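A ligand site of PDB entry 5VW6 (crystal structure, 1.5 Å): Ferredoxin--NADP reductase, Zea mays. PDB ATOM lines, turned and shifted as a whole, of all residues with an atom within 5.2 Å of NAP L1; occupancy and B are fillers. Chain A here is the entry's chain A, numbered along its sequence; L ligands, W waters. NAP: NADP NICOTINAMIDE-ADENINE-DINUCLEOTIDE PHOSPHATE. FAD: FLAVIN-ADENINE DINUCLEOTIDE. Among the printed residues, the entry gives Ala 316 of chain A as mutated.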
ATOM      1  N   PRO A  50     -36.047  12.261  -4.973  1.00  0.00           N
ATOM      2  CA  PRO A  50     -36.900  11.453  -4.084  1.00  0.00           C
ATOM      3  C   PRO A  50     -37.318  12.166  -2.795  1.00  0.00           C
ATOM      4  O   PRO A  50     -38.230  11.676  -2.117  1.00  0.00           O
ATOM      5  CB  PRO A  50     -36.030  10.233  -3.768  1.00  0.00           C
ATOM      6  CG  PRO A  50     -34.634  10.683  -4.022  1.00  0.00           C
ATOM      7  CD  PRO A  50     -34.725  11.639  -5.177  1.00  0.00           C
ATOM      8  N   THR A  53     -34.027  18.323  -0.182  1.00  0.00           N
ATOM      9  CA  THR A  53     -32.855  18.747   0.549  1.00  0.00           C
ATOM     10  C   THR A  53     -32.832  20.257   0.454  1.00  0.00           C
ATOM     11  O   THR A  53     -32.958  20.822  -0.635  1.00  0.00           O
ATOM     12  CB  THR A  53     -31.577  18.150  -0.023  1.00  0.00           C
ATOM     13  OG1 THR A  53     -31.648  16.725   0.117  1.00  0.00           O
ATOM     14  CG2 THR A  53     -30.354  18.667   0.688  1.00  0.00           C
ATOM     15  N   SER A  71     -19.379  20.478  12.584  1.00  0.00           N
ATOM     16  CA  SER A  71     -20.828  20.402  12.623  1.00  0.00           C
ATOM     17  C   SER A  71     -21.377  21.437  13.599  1.00  0.00           C
ATOM     18  O   SER A  71     -20.743  21.781  14.597  1.00  0.00           O
ATOM     19  CB  SER A  71     -21.316  19.015  13.079  1.00  0.00           C
ATOM     20  OG  SER A  71     -21.067  18.040  12.066  1.00  0.00           O
ATOM     21  N   SER A  94     -23.413  18.688   9.480  1.00  0.00           N
ATOM     22  CA  SER A  94     -22.164  19.176   8.933  1.00  0.00           C
ATOM     23  C   SER A  94     -22.363  20.546   8.330  1.00  0.00           C
ATOM     24  O   SER A  94     -23.220  20.751   7.483  1.00  0.00           O
ATOM     25  CB  SER A  94     -21.618  18.237   7.864  1.00  0.00           C
ATOM     26  OG  SER A  94     -21.096  17.075   8.454  1.00  0.00           O
ATOM     27  N   ARG A 114     -31.477  17.137   4.441  1.00  0.00           N
ATOM     28  CA  ARG A 114     -32.494  16.315   3.798  1.00  0.00           C
ATOM     29  C   ARG A 114     -33.662  16.084   4.740  1.00  0.00           C
ATOM     30  O   ARG A 114     -33.458  15.642   5.875  1.00  0.00           O
ATOM     31  CB  ARG A 114     -31.884  14.984   3.367  1.00  0.00           C
ATOM     32  CG  ARG A 114     -32.851  13.921   2.865  1.00  0.00           C
ATOM     33  CD  ARG A 114     -33.490  14.290   1.565  1.00  0.00           C
ATOM     34  NE  ARG A 114     -34.246  13.153   1.043  1.00  0.00           N
ATOM     35  CZ  ARG A 114     -33.764  12.232   0.206  1.00  0.00           C
ATOM     36  NH1 ARG A 114     -34.540  11.231  -0.176  1.00  0.00           N
ATOM     37  NH2 ARG A 114     -32.521  12.311  -0.258  1.00  0.00           N
ATOM     38  N   THR A 173     -21.910  11.113  -0.357  1.00  0.00           N
ATOM     39  CA  THR A 173     -23.249  10.720  -0.781  1.00  0.00           C
ATOM     40  C   THR A 173     -24.251  11.701  -0.200  1.00  0.00           C
ATOM     41  O   THR A 173     -24.220  11.971   1.012  1.00  0.00           O
ATOM     42  CB  THR A 173     -23.599   9.280  -0.376  1.00  0.00           C
ATOM     43  OG1 THR A 173     -23.236   9.058   0.982  1.00  0.00           O
ATOM     44  CG2 THR A 173     -22.886   8.330  -1.288  1.00  0.00           C
ATOM     45  N   GLY A 174     -25.142  12.188  -1.050  1.00  0.00           N
ATOM     46  CA  GLY A 174     -26.197  13.090  -0.621  1.00  0.00           C
ATOM     47  C   GLY A 174     -25.678  14.271   0.169  1.00  0.00           C
ATOM     48  O   GLY A 174     -24.696  14.931  -0.220  1.00  0.00           O
ATOM     49  N   THR A 175     -26.305  14.538   1.309  1.00  0.00           N
ATOM     50  CA  THR A 175     -25.915  15.692   2.119  1.00  0.00           C
ATOM     51  C   THR A 175     -24.520  15.552   2.711  1.00  0.00           C
ATOM     52  O   THR A 175     -24.021  16.519   3.287  1.00  0.00           O
ATOM     53  CB  THR A 175     -26.916  15.921   3.246  1.00  0.00           C
ATOM     54  OG1 THR A 175     -27.020  14.742   4.043  1.00  0.00           O
ATOM     55  CG2 THR A 175     -28.281  16.259   2.706  1.00  0.00           C
ATOM     56  N   GLY A 176     -23.897  14.382   2.577  1.00  0.00           N
ATOM     57  CA  GLY A 176     -22.490  14.237   2.914  1.00  0.00           C
ATOM     58  C   GLY A 176     -21.593  15.173   2.125  1.00  0.00           C
ATOM     59  O   GLY A 176     -20.419  15.353   2.479  1.00  0.00           O
ATOM     60  N   ALA A 178     -21.749  18.202   2.310  1.00  0.00           N
ATOM     61  CA  ALA A 178     -21.724  19.415   3.093  1.00  0.00           C
ATOM     62  C   ALA A 178     -20.317  19.910   3.413  1.00  0.00           C
ATOM     63  O   ALA A 178     -19.948  21.029   3.043  1.00  0.00           O
ATOM     64  CB  ALA A 178     -22.511  19.222   4.381  1.00  0.00           C
ATOM     65  N   PRO A 179     -19.487  19.123   4.087  1.00  0.00           N
ATOM     66  CA  PRO A 179     -18.152  19.649   4.437  1.00  0.00           C
ATOM     67  C   PRO A 179     -17.371  20.037   3.195  1.00  0.00           C
ATOM     68  O   PRO A 179     -16.562  20.968   3.219  1.00  0.00           O
ATOM     69  CB  PRO A 179     -17.485  18.497   5.167  1.00  0.00           C
ATOM     70  CG  PRO A 179     -18.205  17.286   4.651  1.00  0.00           C
ATOM     71  CD  PRO A 179     -19.623  17.725   4.500  1.00  0.00           C
ATOM     72  N   GLY A 206     -22.325  11.168  -5.031  1.00  0.00           N
ATOM     73  CA  GLY A 206     -23.388  10.257  -5.382  1.00  0.00           C
ATOM     74  C   GLY A 206     -24.730  10.814  -4.920  1.00  0.00           C
ATOM     75  O   GLY A 206     -24.890  11.167  -3.752  1.00  0.00           O
ATOM     76  N   VAL A 207     -25.649  10.944  -5.877  1.00  0.00           N
ATOM     77  CA  VAL A 207     -27.021  11.354  -5.599  1.00  0.00           C
ATOM     78  C   VAL A 207     -27.952  10.547  -6.498  1.00  0.00           C
ATOM     79  O   VAL A 207     -27.520   9.904  -7.447  1.00  0.00           O
ATOM     80  CB  VAL A 207     -27.246  12.857  -5.808  1.00  0.00           C
ATOM     81  CG1 VAL A 207     -26.380  13.617  -4.827  1.00  0.00           C
ATOM     82  CG2 VAL A 207     -26.970  13.235  -7.246  1.00  0.00           C
ATOM     83  N   ALA A 208     -29.238  10.560  -6.152  1.00  0.00           N
ATOM     84  CA  ALA A 208     -30.193   9.673  -6.813  1.00  0.00           C
ATOM     85  C   ALA A 208     -30.309   9.963  -8.301  1.00  0.00           C
ATOM     86  O   ALA A 208     -30.372   9.030  -9.116  1.00  0.00           O
ATOM     87  CB  ALA A 208     -31.577   9.809  -6.162  1.00  0.00           C
ATOM     88  N   ALA A 235     -22.038  10.141  -9.428  1.00  0.00           N
ATOM     89  CA  ALA A 235     -22.682   8.838  -9.558  1.00  0.00           C
ATOM     90  C   ALA A 235     -24.169   9.060  -9.328  1.00  0.00           C
ATOM     91  O   ALA A 235     -24.582   9.331  -8.201  1.00  0.00           O
ATOM     92  CB  ALA A 235     -22.097   7.842  -8.578  1.00  0.00           C
ATOM     93  N   SER A 237     -27.438   7.378  -9.010  1.00  0.00           N
ATOM     94  CA  SER A 237     -27.744   5.985  -8.734  1.00  0.00           C
ATOM     95  C   SER A 237     -28.993   5.512  -9.462  1.00  0.00           C
ATOM     96  O   SER A 237     -29.082   4.338  -9.832  1.00  0.00           O
ATOM     97  CB  SER A 237     -27.920   5.770  -7.234  1.00  0.00           C
ATOM     98  OG  SER A 237     -28.988   6.569  -6.760  1.00  0.00           O
ATOM     99  N   ARG A 238     -29.966   6.399  -9.673  1.00  0.00           N
ATOM    100  CA  ARG A 238     -31.214   6.036 -10.334  1.00  0.00           C
ATOM    101  C   ARG A 238     -31.222   6.435 -11.810  1.00  0.00           C
ATOM    102  O   ARG A 238     -32.238   6.231 -12.491  1.00  0.00           O
ATOM    103  CB  ARG A 238     -32.391   6.631  -9.564  1.00  0.00           C
ATOM    104  CG  ARG A 238     -32.389   6.153  -8.115  1.00  0.00           C
ATOM    105  CD  ARG A 238     -33.515   6.690  -7.250  1.00  0.00           C
ATOM    106  NE  ARG A 238     -33.276   6.341  -5.851  1.00  0.00           N
ATOM    107  CZ  ARG A 238     -34.170   6.438  -4.878  1.00  0.00           C
ATOM    108  NH1 ARG A 238     -35.397   6.873  -5.139  1.00  0.00           N
ATOM    109  NH2 ARG A 238     -33.839   6.099  -3.644  1.00  0.00           N
ATOM    110  N   LYS A 247     -26.943  -0.271  -9.151  1.00  0.00           N
ATOM    111  CA  LYS A 247     -27.057   1.155  -9.375  1.00  0.00           C
ATOM    112  C   LYS A 247     -25.686   1.799  -9.317  1.00  0.00           C
ATOM    113  O   LYS A 247     -24.795   1.350  -8.590  1.00  0.00           O
ATOM    114  CB  LYS A 247     -27.996   1.787  -8.339  1.00  0.00           C
ATOM    115  CG  LYS A 247     -29.447   1.354  -8.472  1.00  0.00           C
ATOM    116  CD  LYS A 247     -30.393   2.287  -7.716  1.00  0.00           C
ATOM    117  CE  LYS A 247     -30.537   1.897  -6.257  1.00  0.00           C
ATOM    118  NZ  LYS A 247     -31.806   2.437  -5.674  1.00  0.00           N
ATOM    119  N   TYR A 249     -23.073   3.836  -8.028  1.00  0.00           N
ATOM    120  CA  TYR A 249     -22.765   4.393  -6.724  1.00  0.00           C
ATOM    121  C   TYR A 249     -21.354   5.000  -6.752  1.00  0.00           C
ATOM    122  O   TYR A 249     -20.597   4.819  -7.712  1.00  0.00           O
ATOM    123  CB  TYR A 249     -22.870   3.290  -5.656  1.00  0.00           C
ATOM    124  CG  TYR A 249     -24.282   2.946  -5.160  1.00  0.00           C
ATOM    125  CD1 TYR A 249     -25.372   3.780  -5.391  1.00  0.00           C
ATOM    126  CD2 TYR A 249     -24.508   1.778  -4.416  1.00  0.00           C
ATOM    127  CE1 TYR A 249     -26.647   3.469  -4.916  1.00  0.00           C
ATOM    128  CE2 TYR A 249     -25.782   1.467  -3.941  1.00  0.00           C
ATOM    129  CZ  TYR A 249     -26.843   2.312  -4.177  1.00  0.00           C
ATOM    130  OH  TYR A 249     -28.103   2.000  -3.705  1.00  0.00           O
ATOM    131  N   VAL A 250     -21.003   5.769  -5.713  1.00  0.00           N
ATOM    132  CA  VAL A 250     -19.690   6.424  -5.707  1.00  0.00           C
ATOM    133  C   VAL A 250     -18.563   5.394  -5.799  1.00  0.00           C
ATOM    134  O   VAL A 250     -17.533   5.653  -6.428  1.00  0.00           O
ATOM    135  CB  VAL A 250     -19.505   7.326  -4.485  1.00  0.00           C
ATOM    136  CG1 VAL A 250     -20.344   8.579  -4.614  1.00  0.00           C
ATOM    137  CG2 VAL A 250     -19.796   6.631  -3.187  1.00  0.00           C
ATOM    138  N   GLN A 251     -18.744   4.222  -5.194  1.00  0.00           N
ATOM    139  CA  GLN A 251     -17.678   3.215  -5.227  1.00  0.00           C
ATOM    140  C   GLN A 251     -17.403   2.760  -6.653  1.00  0.00           C
ATOM    141  O   GLN A 251     -16.257   2.485  -7.011  1.00  0.00           O
ATOM    142  CB  GLN A 251     -18.021   2.017  -4.333  1.00  0.00           C
ATOM    143  CG  GLN A 251     -19.434   1.483  -4.418  1.00  0.00           C
ATOM    144  CD  GLN A 251     -20.360   2.168  -3.436  1.00  0.00           C
ATOM    145  OE1 GLN A 251     -20.249   3.361  -3.222  1.00  0.00           O
ATOM    146  NE2 GLN A 251     -21.271   1.417  -2.833  1.00  0.00           N
ATOM    147  N   CYS A 274     -17.974  11.209   3.495  1.00  0.00           N
ATOM    148  CA  CYS A 274     -19.023  11.827   4.285  1.00  0.00           C
ATOM    149  C   CYS A 274     -20.363  11.517   3.647  1.00  0.00           C
ATOM    150  O   CYS A 274     -20.504  11.608   2.431  1.00  0.00           O
ATOM    151  CB  CYS A 274     -18.807  13.345   4.373  1.00  0.00           C
ATOM    152  SG  CYS A 274     -19.897  14.122   5.590  1.00  0.00           S
ATOM    153  N   GLY A 275     -21.332  11.124   4.452  1.00  0.00           N
ATOM    154  CA  GLY A 275     -22.633  10.794   3.940  1.00  0.00           C
ATOM    155  C   GLY A 275     -23.188   9.575   4.633  1.00  0.00           C
ATOM    156  O   GLY A 275     -23.019   9.417   5.846  1.00  0.00           O
ATOM    157  N   LEU A 276     -23.853   8.737   3.856  1.00  0.00           N
ATOM    158  CA  LEU A 276     -24.532   7.552   4.366  1.00  0.00           C
ATOM    159  C   LEU A 276     -23.543   6.566   4.961  1.00  0.00           C
ATOM    160  O   LEU A 276     -22.586   6.170   4.300  1.00  0.00           O
ATOM    161  CB  LEU A 276     -25.287   6.844   3.225  1.00  0.00           C
ATOM    162  CG  LEU A 276     -26.473   7.505   2.526  1.00  0.00           C
ATOM    163  CD1 LEU A 276     -26.690   6.871   1.170  1.00  0.00           C
ATOM    164  CD2 LEU A 276     -27.734   7.350   3.359  1.00  0.00           C
ATOM    165  N   GLY A 278     -23.978   3.582   5.168  1.00  0.00           N
ATOM    166  CA  GLY A 278     -24.087   2.365   4.408  1.00  0.00           C
ATOM    167  C   GLY A 278     -23.208   2.330   3.183  1.00  0.00           C
ATOM    168  O   GLY A 278     -23.068   1.257   2.584  1.00  0.00           O
ATOM    169  N   MET A 279     -22.617   3.460   2.800  1.00  0.00           N
ATOM    170  CA  MET A 279     -21.741   3.429   1.646  1.00  0.00           C
ATOM    171  C   MET A 279     -20.370   2.846   1.980  1.00  0.00           C
ATOM    172  O   MET A 279     -19.692   2.341   1.071  1.00  0.00           O
ATOM    173  CB  MET A 279     -21.589   4.809   1.019  1.00  0.00           C
ATOM    174  CG  MET A 279     -20.694   5.741   1.769  1.00  0.00           C
ATOM    175  SD  MET A 279     -20.452   7.242   0.882  1.00  0.00           S
ATOM    176  CE  MET A 279     -19.876   8.117   2.289  1.00  0.00           C
ATOM    177  N   GLU A 314     -16.586  10.488   8.221  1.00  0.00           N
ATOM    178  CA  GLU A 314     -17.683  10.894   9.095  1.00  0.00           C
ATOM    179  C   GLU A 314     -18.974  10.540   8.380  1.00  0.00           C
ATOM    180  O   GLU A 314     -19.350  11.179   7.387  1.00  0.00           O
ATOM    181  CB  GLU A 314     -17.620  12.383   9.430  1.00  0.00           C
ATOM    182  CG  GLU A 314     -17.395  12.670  10.865  1.00  0.00           C
ATOM    183  CD  GLU A 314     -17.445  14.148  11.177  1.00  0.00           C
ATOM    184  OE1 GLU A 314     -18.412  14.827  10.779  1.00  0.00           O
ATOM    185  OE2 GLU A 314     -16.489  14.641  11.808  1.00  0.00           O
ATOM    186  N   VAL A 315     -19.668   9.512   8.857  1.00  0.00           N
ATOM    187  CA  VAL A 315     -20.854   9.034   8.169  1.00  0.00           C
ATOM    188  C   VAL A 315     -21.908   8.767   9.227  1.00  0.00           C
ATOM    189  O   VAL A 315     -21.601   8.593  10.409  1.00  0.00           O
ATOM    190  CB  VAL A 315     -20.586   7.779   7.313  1.00  0.00           C
ATOM    191  CG1 VAL A 315     -19.597   8.078   6.183  1.00  0.00           C
ATOM    192  CG2 VAL A 315     -20.044   6.610   8.142  1.00  0.00           C
ATOM    193  N   ALA A 316     -23.164   8.749   8.780  1.00  0.00           N
ATOM    194  CA  ALA A 316     -24.288   8.568   9.684  1.00  0.00           C
ATOM    195  C   ALA A 316     -25.478   8.003   8.939  1.00  0.00           C
ATOM    196  O   ALA A 316     -25.514   8.025   7.709  1.00  0.00           O
ATOM    197  CB  ALA A 316     -24.660   9.889  10.322  1.00  0.00           C
ATOM    198  OXT ALA A 316     -26.446   7.560   9.593  1.00  0.00           O
HETATM  199  PA  NAP L   1     -29.666   9.640  -0.042  1.00  0.00           P
HETATM  200  O1A NAP L   1     -30.416  10.337  -1.121  1.00  0.00           O
HETATM  201  O2A NAP L   1     -30.340   8.628   0.856  1.00  0.00           O
HETATM  202  O5B NAP L   1     -28.509   8.848  -0.793  1.00  0.00           O
HETATM  203  C5B NAP L   1     -27.572   9.633  -1.533  1.00  0.00           C
HETATM  204  C4B NAP L   1     -27.003   8.727  -2.617  1.00  0.00           C
HETATM  205  O4B NAP L   1     -26.300   7.643  -2.036  1.00  0.00           O
HETATM  206  C3B NAP L   1     -28.117   8.114  -3.443  1.00  0.00           C
HETATM  207  O3B NAP L   1     -27.709   8.025  -4.798  1.00  0.00           O
HETATM  208  C2B NAP L   1     -28.270   6.707  -2.947  1.00  0.00           C
HETATM  209  O2B NAP L   1     -28.756   5.813  -3.931  1.00  0.00           O
HETATM  210  C1B NAP L   1     -26.802   6.447  -2.646  1.00  0.00           C
HETATM  211  N9A NAP L   1     -26.627   5.231  -1.841  1.00  0.00           N
HETATM  212  C8A NAP L   1     -27.552   4.550  -1.146  1.00  0.00           C
HETATM  213  N7A NAP L   1     -26.990   3.460  -0.584  1.00  0.00           N
HETATM  214  C5A NAP L   1     -25.700   3.440  -0.941  1.00  0.00           C
HETATM  215  C6A NAP L   1     -24.542   2.556  -0.698  1.00  0.00           C
HETATM  216  N6A NAP L   1     -24.643   1.446   0.065  1.00  0.00           N
HETATM  217  N1A NAP L   1     -23.377   2.917  -1.269  1.00  0.00           N
HETATM  218  C2A NAP L   1     -23.236   4.007  -2.038  1.00  0.00           C
HETATM  219  N3A NAP L   1     -24.249   4.854  -2.292  1.00  0.00           N
HETATM  220  C4A NAP L   1     -25.476   4.603  -1.786  1.00  0.00           C
HETATM  221  O3  NAP L   1     -28.737  10.657   0.781  1.00  0.00           O
HETATM  222  PN  NAP L   1     -29.178  11.604   1.966  1.00  0.00           P
HETATM  223  O1N NAP L   1     -30.641  11.350   2.296  1.00  0.00           O
HETATM  224  O2N NAP L   1     -28.616  12.969   1.692  1.00  0.00           O
HETATM  225  O5D NAP L   1     -28.349  10.874   3.125  1.00  0.00           O
HETATM  226  C5D NAP L   1     -27.071  11.364   3.504  1.00  0.00           C
HETATM  227  C4D NAP L   1     -26.647  10.661   4.774  1.00  0.00           C
HETATM  228  O4D NAP L   1     -25.410  11.243   5.188  1.00  0.00           O
HETATM  229  C3D NAP L   1     -27.624  10.803   5.930  1.00  0.00           C
HETATM  230  O3D NAP L   1     -27.781   9.500   6.516  1.00  0.00           O
HETATM  231  C2D NAP L   1     -26.928  11.779   6.861  1.00  0.00           C
HETATM  232  O2D NAP L   1     -27.156  11.522   8.238  1.00  0.00           O
HETATM  233  C1D NAP L   1     -25.460  11.522   6.574  1.00  0.00           C
HETATM  234  N1N NAP L   1     -24.591  12.662   6.796  1.00  0.00           N
HETATM  235  C2N NAP L   1     -23.635  12.518   7.677  1.00  0.00           C
HETATM  236  C3N NAP L   1     -22.755  13.550   7.910  1.00  0.00           C
HETATM  237  C7N NAP L   1     -21.721  13.340   8.933  1.00  0.00           C
HETATM  238  O7N NAP L   1     -21.654  12.277   9.528  1.00  0.00           O
HETATM  239  N7N NAP L   1     -20.820  14.271   9.186  1.00  0.00           N
HETATM  240  C4N NAP L   1     -22.875  14.736   7.198  1.00  0.00           C
HETATM  241  C5N NAP L   1     -23.868  14.844   6.243  1.00  0.00           C
HETATM  242  C6N NAP L   1     -24.706  13.766   6.035  1.00  0.00           C
HETATM  243  P2B NAP L   1     -30.242   5.152  -3.830  1.00  0.00           P
HETATM  244  O1X NAP L   1     -30.709   5.248  -5.259  1.00  0.00           O
HETATM  245  O2X NAP L   1     -29.970   3.717  -3.407  1.00  0.00           O
HETATM  246  O3X NAP L   1     -31.046   5.945  -2.839  1.00  0.00           O
HETATM  247  PA  FAD L   2     -35.538  12.182  14.115  1.00  0.00           P
HETATM  248  O1A FAD L   2     -36.828  12.847  14.556  1.00  0.00           O
HETATM  249  O2A FAD L   2     -34.340  12.127  15.007  1.00  0.00           O
HETATM  250  O5B FAD L   2     -35.926  10.740  13.545  1.00  0.00           O
HETATM  251  C5B FAD L   2     -34.902   9.868  13.069  1.00  0.00           C
HETATM  252  C4B FAD L   2     -35.464   8.949  11.985  1.00  0.00           C
HETATM  253  O4B FAD L   2     -36.465   8.092  12.545  1.00  0.00           O
HETATM  254  C3B FAD L   2     -36.145   9.729  10.864  1.00  0.00           C
HETATM  255  O3B FAD L   2     -35.781   9.123   9.621  1.00  0.00           O
HETATM  256  C2B FAD L   2     -37.626   9.553  11.153  1.00  0.00           C
HETATM  257  O2B FAD L   2     -38.460   9.615   9.993  1.00  0.00           O
HETATM  258  C1B FAD L   2     -37.665   8.174  11.763  1.00  0.00           C
HETATM  259  N9A FAD L   2     -38.789   7.930  12.669  1.00  0.00           N
HETATM  260  C8A FAD L   2     -39.250   8.741  13.637  1.00  0.00           C
HETATM  261  N7A FAD L   2     -40.289   8.155  14.266  1.00  0.00           N
HETATM  262  C5A FAD L   2     -40.470   6.954  13.689  1.00  0.00           C
HETATM  263  C6A FAD L   2     -41.393   5.823  13.869  1.00  0.00           C
HETATM  264  N6A FAD L   2     -42.326   5.916  14.828  1.00  0.00           N
HETATM  265  N1A FAD L   2     -41.247   4.747  13.067  1.00  0.00           N
HETATM  266  C2A FAD L   2     -40.312   4.682  12.097  1.00  0.00           C
HETATM  267  N3A FAD L   2     -39.443   5.696  11.887  1.00  0.00           N
HETATM  268  C4A FAD L   2     -39.489   6.816  12.643  1.00  0.00           C
HETATM  269  N1  FAD L   2     -28.239  15.196   8.171  1.00  0.00           N
HETATM  270  C2  FAD L   2     -28.398  16.060   7.160  1.00  0.00           C
HETATM  271  O2  FAD L   2     -29.497  16.103   6.557  1.00  0.00           O
HETATM  272  N3  FAD L   2     -27.398  16.851   6.744  1.00  0.00           N
HETATM  273  C4  FAD L   2     -26.180  16.921   7.286  1.00  0.00           C
HETATM  274  O4  FAD L   2     -25.279  17.695   6.886  1.00  0.00           O
HETATM  275  C4X FAD L   2     -25.941  16.033   8.417  1.00  0.00           C
HETATM  276  N5  FAD L   2     -24.753  15.981   9.048  1.00  0.00           N
HETATM  277  C5X FAD L   2     -24.624  15.189  10.143  1.00  0.00           C
HETATM  278  C6  FAD L   2     -23.428  15.225  10.851  1.00  0.00           C
HETATM  279  C7  FAD L   2     -23.204  14.334  11.883  1.00  0.00           C
HETATM  280  C7M FAD L   2     -21.885  14.351  12.613  1.00  0.00           C
HETATM  281  C8  FAD L   2     -24.224  13.365  12.256  1.00  0.00           C
HETATM  282  C8M FAD L   2     -23.990  12.398  13.370  1.00  0.00           C
HETATM  283  C9  FAD L   2     -25.428  13.345  11.579  1.00  0.00           C
HETATM  284  C9A FAD L   2     -25.672  14.245  10.550  1.00  0.00           C
HETATM  285  N10 FAD L   2     -26.887  14.232   9.834  1.00  0.00           N
HETATM  286  C10 FAD L   2     -27.054  15.153   8.822  1.00  0.00           C
HETATM  287  C1' FAD L   2     -28.086  13.558  10.327  1.00  0.00           C
HETATM  288  C2' FAD L   2     -28.834  14.486  11.306  1.00  0.00           C
HETATM  289  O2' FAD L   2     -28.043  14.722  12.475  1.00  0.00           O
HETATM  290  C3' FAD L   2     -30.162  13.889  11.787  1.00  0.00           C
HETATM  291  O3' FAD L   2     -29.947  12.597  12.396  1.00  0.00           O
HETATM  292  C4' FAD L   2     -31.186  13.810  10.669  1.00  0.00           C
HETATM  293  O4' FAD L   2     -31.416  15.139  10.223  1.00  0.00           O
HETATM  294  C5' FAD L   2     -32.498  13.248  11.187  1.00  0.00           C
HETATM  295  O5' FAD L   2     -32.898  13.907  12.393  1.00  0.00           O
HETATM  296  P   FAD L   2     -34.424  14.316  12.603  1.00  0.00           P
HETATM  297  O1P FAD L   2     -34.488  15.078  13.908  1.00  0.00           O
HETATM  298  O2P FAD L   2     -34.992  14.929  11.357  1.00  0.00           O
HETATM  299  O3P FAD L   2     -35.084  12.835  12.743  1.00  0.00           O
HETATM  300  O   HOH W   1     -29.727  11.643  -3.406  1.00  0.00           O
HETATM  301  O   HOH W   2     -25.169   7.595  -6.061  1.00  0.00           O
HETATM  302  O   HOH W   3     -31.951   8.646  -2.735  1.00  0.00           O
HETATM  303  O   HOH W   4     -23.284   6.729  -4.229  1.00  0.00           O
HETATM  304  O   HOH W   5     -32.803   9.855   2.461  1.00  0.00           O
HETATM  305  O   HOH W   6     -28.423   9.625   9.746  1.00  0.00           O
HETATM  306  O   HOH W   7     -27.544   6.118   7.097  1.00  0.00           O
HETATM  307  O   HOH W   8     -29.180  13.691   5.087  1.00  0.00           O
HETATM  308  O   HOH W   9     -30.037   8.144   6.034  1.00  0.00           O
HETATM  309  O   HOH W  10     -30.586   6.133   0.020  1.00  0.00           O
HETATM  310  O   HOH W  11     -20.814  11.026  11.843  1.00  0.00           O
HETATM  311  O   HOH W  12     -31.133  11.386   5.010  1.00  0.00           O
HETATM  312  O   HOH W  13     -31.046   7.714   3.447  1.00  0.00           O
HETATM  313  O   HOH W  14     -29.915  14.655  -0.271  1.00  0.00           O
HETATM  314  O   HOH W  15     -22.176  -0.646   0.517  1.00  0.00           O
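The backbone carbonyl oxygen (O) of Gly 275 is in hydrogen-bond range of the backbone NH (N) of Ala 316 (3.0 Å). The side-chain hydroxyl (OG1) of Thr 173 sits at hydrogen-bond distance from the side-chain sulfur (SD) of Met 279. The backbone carbonyl oxygen of Cys 274 is in hydrogen-bond range of the backbone NH of Thr 173 (3.2 Å). The backbone NH (N) of Arg 238 is in hydrogen-bond range of the backbone carbonyl oxygen (O) of Ala 208, at 2.7 Å. SG of Cys 274 sits close to O of Glu 314 (3.5 Å). O of Val 207 sits at hydrogen-bond distance from N of Ser 237 (3.0 Å). N of Ser 237 sits at hydrogen-bond distance from O of Ala 208, at 3.4 Å. The side-chain sulfur (SG) of Cys 274 sits close to the backbone carbonyl oxygen (O) of Gly 176, at 3.4 Å.
An oxygen (O4D) of NAP L1 sits close to the backbone carbonyl oxygen (O) of Gly 275 (3.1 Å). Residues that only touch NAP L1: Gly 174 (3.3 Å), Met 279 (3.4 Å), Gly 206 (3.4 Å), Thr 173 (3.6 Å) and Gly 176 (3.6 Å). Of the 29 residues printed, 22 come within 4 Å of NAP L1.
Water W6 lies within hydrogen-bond range of O2D of NAP L1 and OXT of Ala 316. Water W11 lies within hydrogen-bond range of an oxygen (O7N) of NAP L1 (2.8 Å) and the backbone carbonyl oxygen of Val 315 (2.9 Å). Water W3 lies within hydrogen-bond range of O1A of NAP L1 (2.8 Å) and NH2 of Arg 238 (3.3 Å). Water W4 bridges a nitrogen (N3A) of NAP L1 (2.9 Å) and the backbone NH (N) of Val 250 (2.9 Å). Water W2 lies within hydrogen-bond range of the backbone carbonyl oxygen (O) of Ala 235 (2.8 Å), an oxygen (O3B) of NAP L1 (2.9 Å) and the backbone NH (N) of Val 207 (3.4 Å). Water W8 bridges the side-chain hydroxyl of Thr 175 and an oxygen (O2) of FAD L2.
A nitrogen (N3) of FAD L2 sits at hydrogen-bond distance from the side-chain hydroxyl (OG1) of Thr 175, at 3.4 Å. An oxygen (O1A) of NAP L1 is in salt-bridge range of the guanidinium group (NH2) of Arg 114, 3.0 Å away. OG1 of Thr 175 sits close to O2N of NAP L1, at 3.3 Å. N6A of NAP L1 is in hydrogen-bond range of O of Gly 278 (3.0 Å). O of Val 207 sits close to O3B of NAP L1, 3.3 Å away. O of Ala 316 lies within hydrogen-bond range of O3D of NAP L1. The backbone NH of Leu 276 lies within hydrogen-bond range of an oxygen (O4D) of NAP L1 (3.2 Å). An oxygen (O1X) of NAP L1 is in salt-bridge range of the guanidinium group (NE) of Arg 238 (2.9 Å). SG of Cys 274 sits close to N7N of NAP L1, 3.7 Å away. The side-chain carboxylate of Glu 314 sits at hydrogen-bond distance from a nitrogen (N7N) of NAP L1. An oxygen (O1X) of NAP L1 lies within hydrogen-bond range of the side-chain hydroxyl (OG) of Ser 237 (2.6 Å). An oxygen (O1X) of NAP L1 is in salt-bridge range of the side-chain amino group (NZ) of Lys 247. The backbone NH of Ala 208 is in hydrogen-bond range of an oxygen (O3B) of NAP L1, at 3.3 Å. O2X of NAP L1 lies within hydrogen-bond range of OH of Tyr 249, at 2.6 Å. The side-chain amide nitrogen (NE2) of Gln 251 is in hydrogen-bond range of a nitrogen (N1A) of NAP L1, 3.0 Å away. N of Arg 114 sits at hydrogen-bond distance from O2 of FAD L2 (3.1 Å). A nitrogen (N5) of FAD L2 lies within hydrogen-bond range of the backbone NH (N) of Ser 94. A nitrogen (N7N) of NAP L1 is in hydrogen-bond range of the side-chain hydroxyl (OG) of Ser 94 (2.9 Å). The backbone NH (N) of Val 315 sits at hydrogen-bond distance from an oxygen (O7N) of NAP L1. The backbone NH of Thr 175 lies within hydrogen-bond range of an oxygen (O2N) of NAP L1 (2.8 Å).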
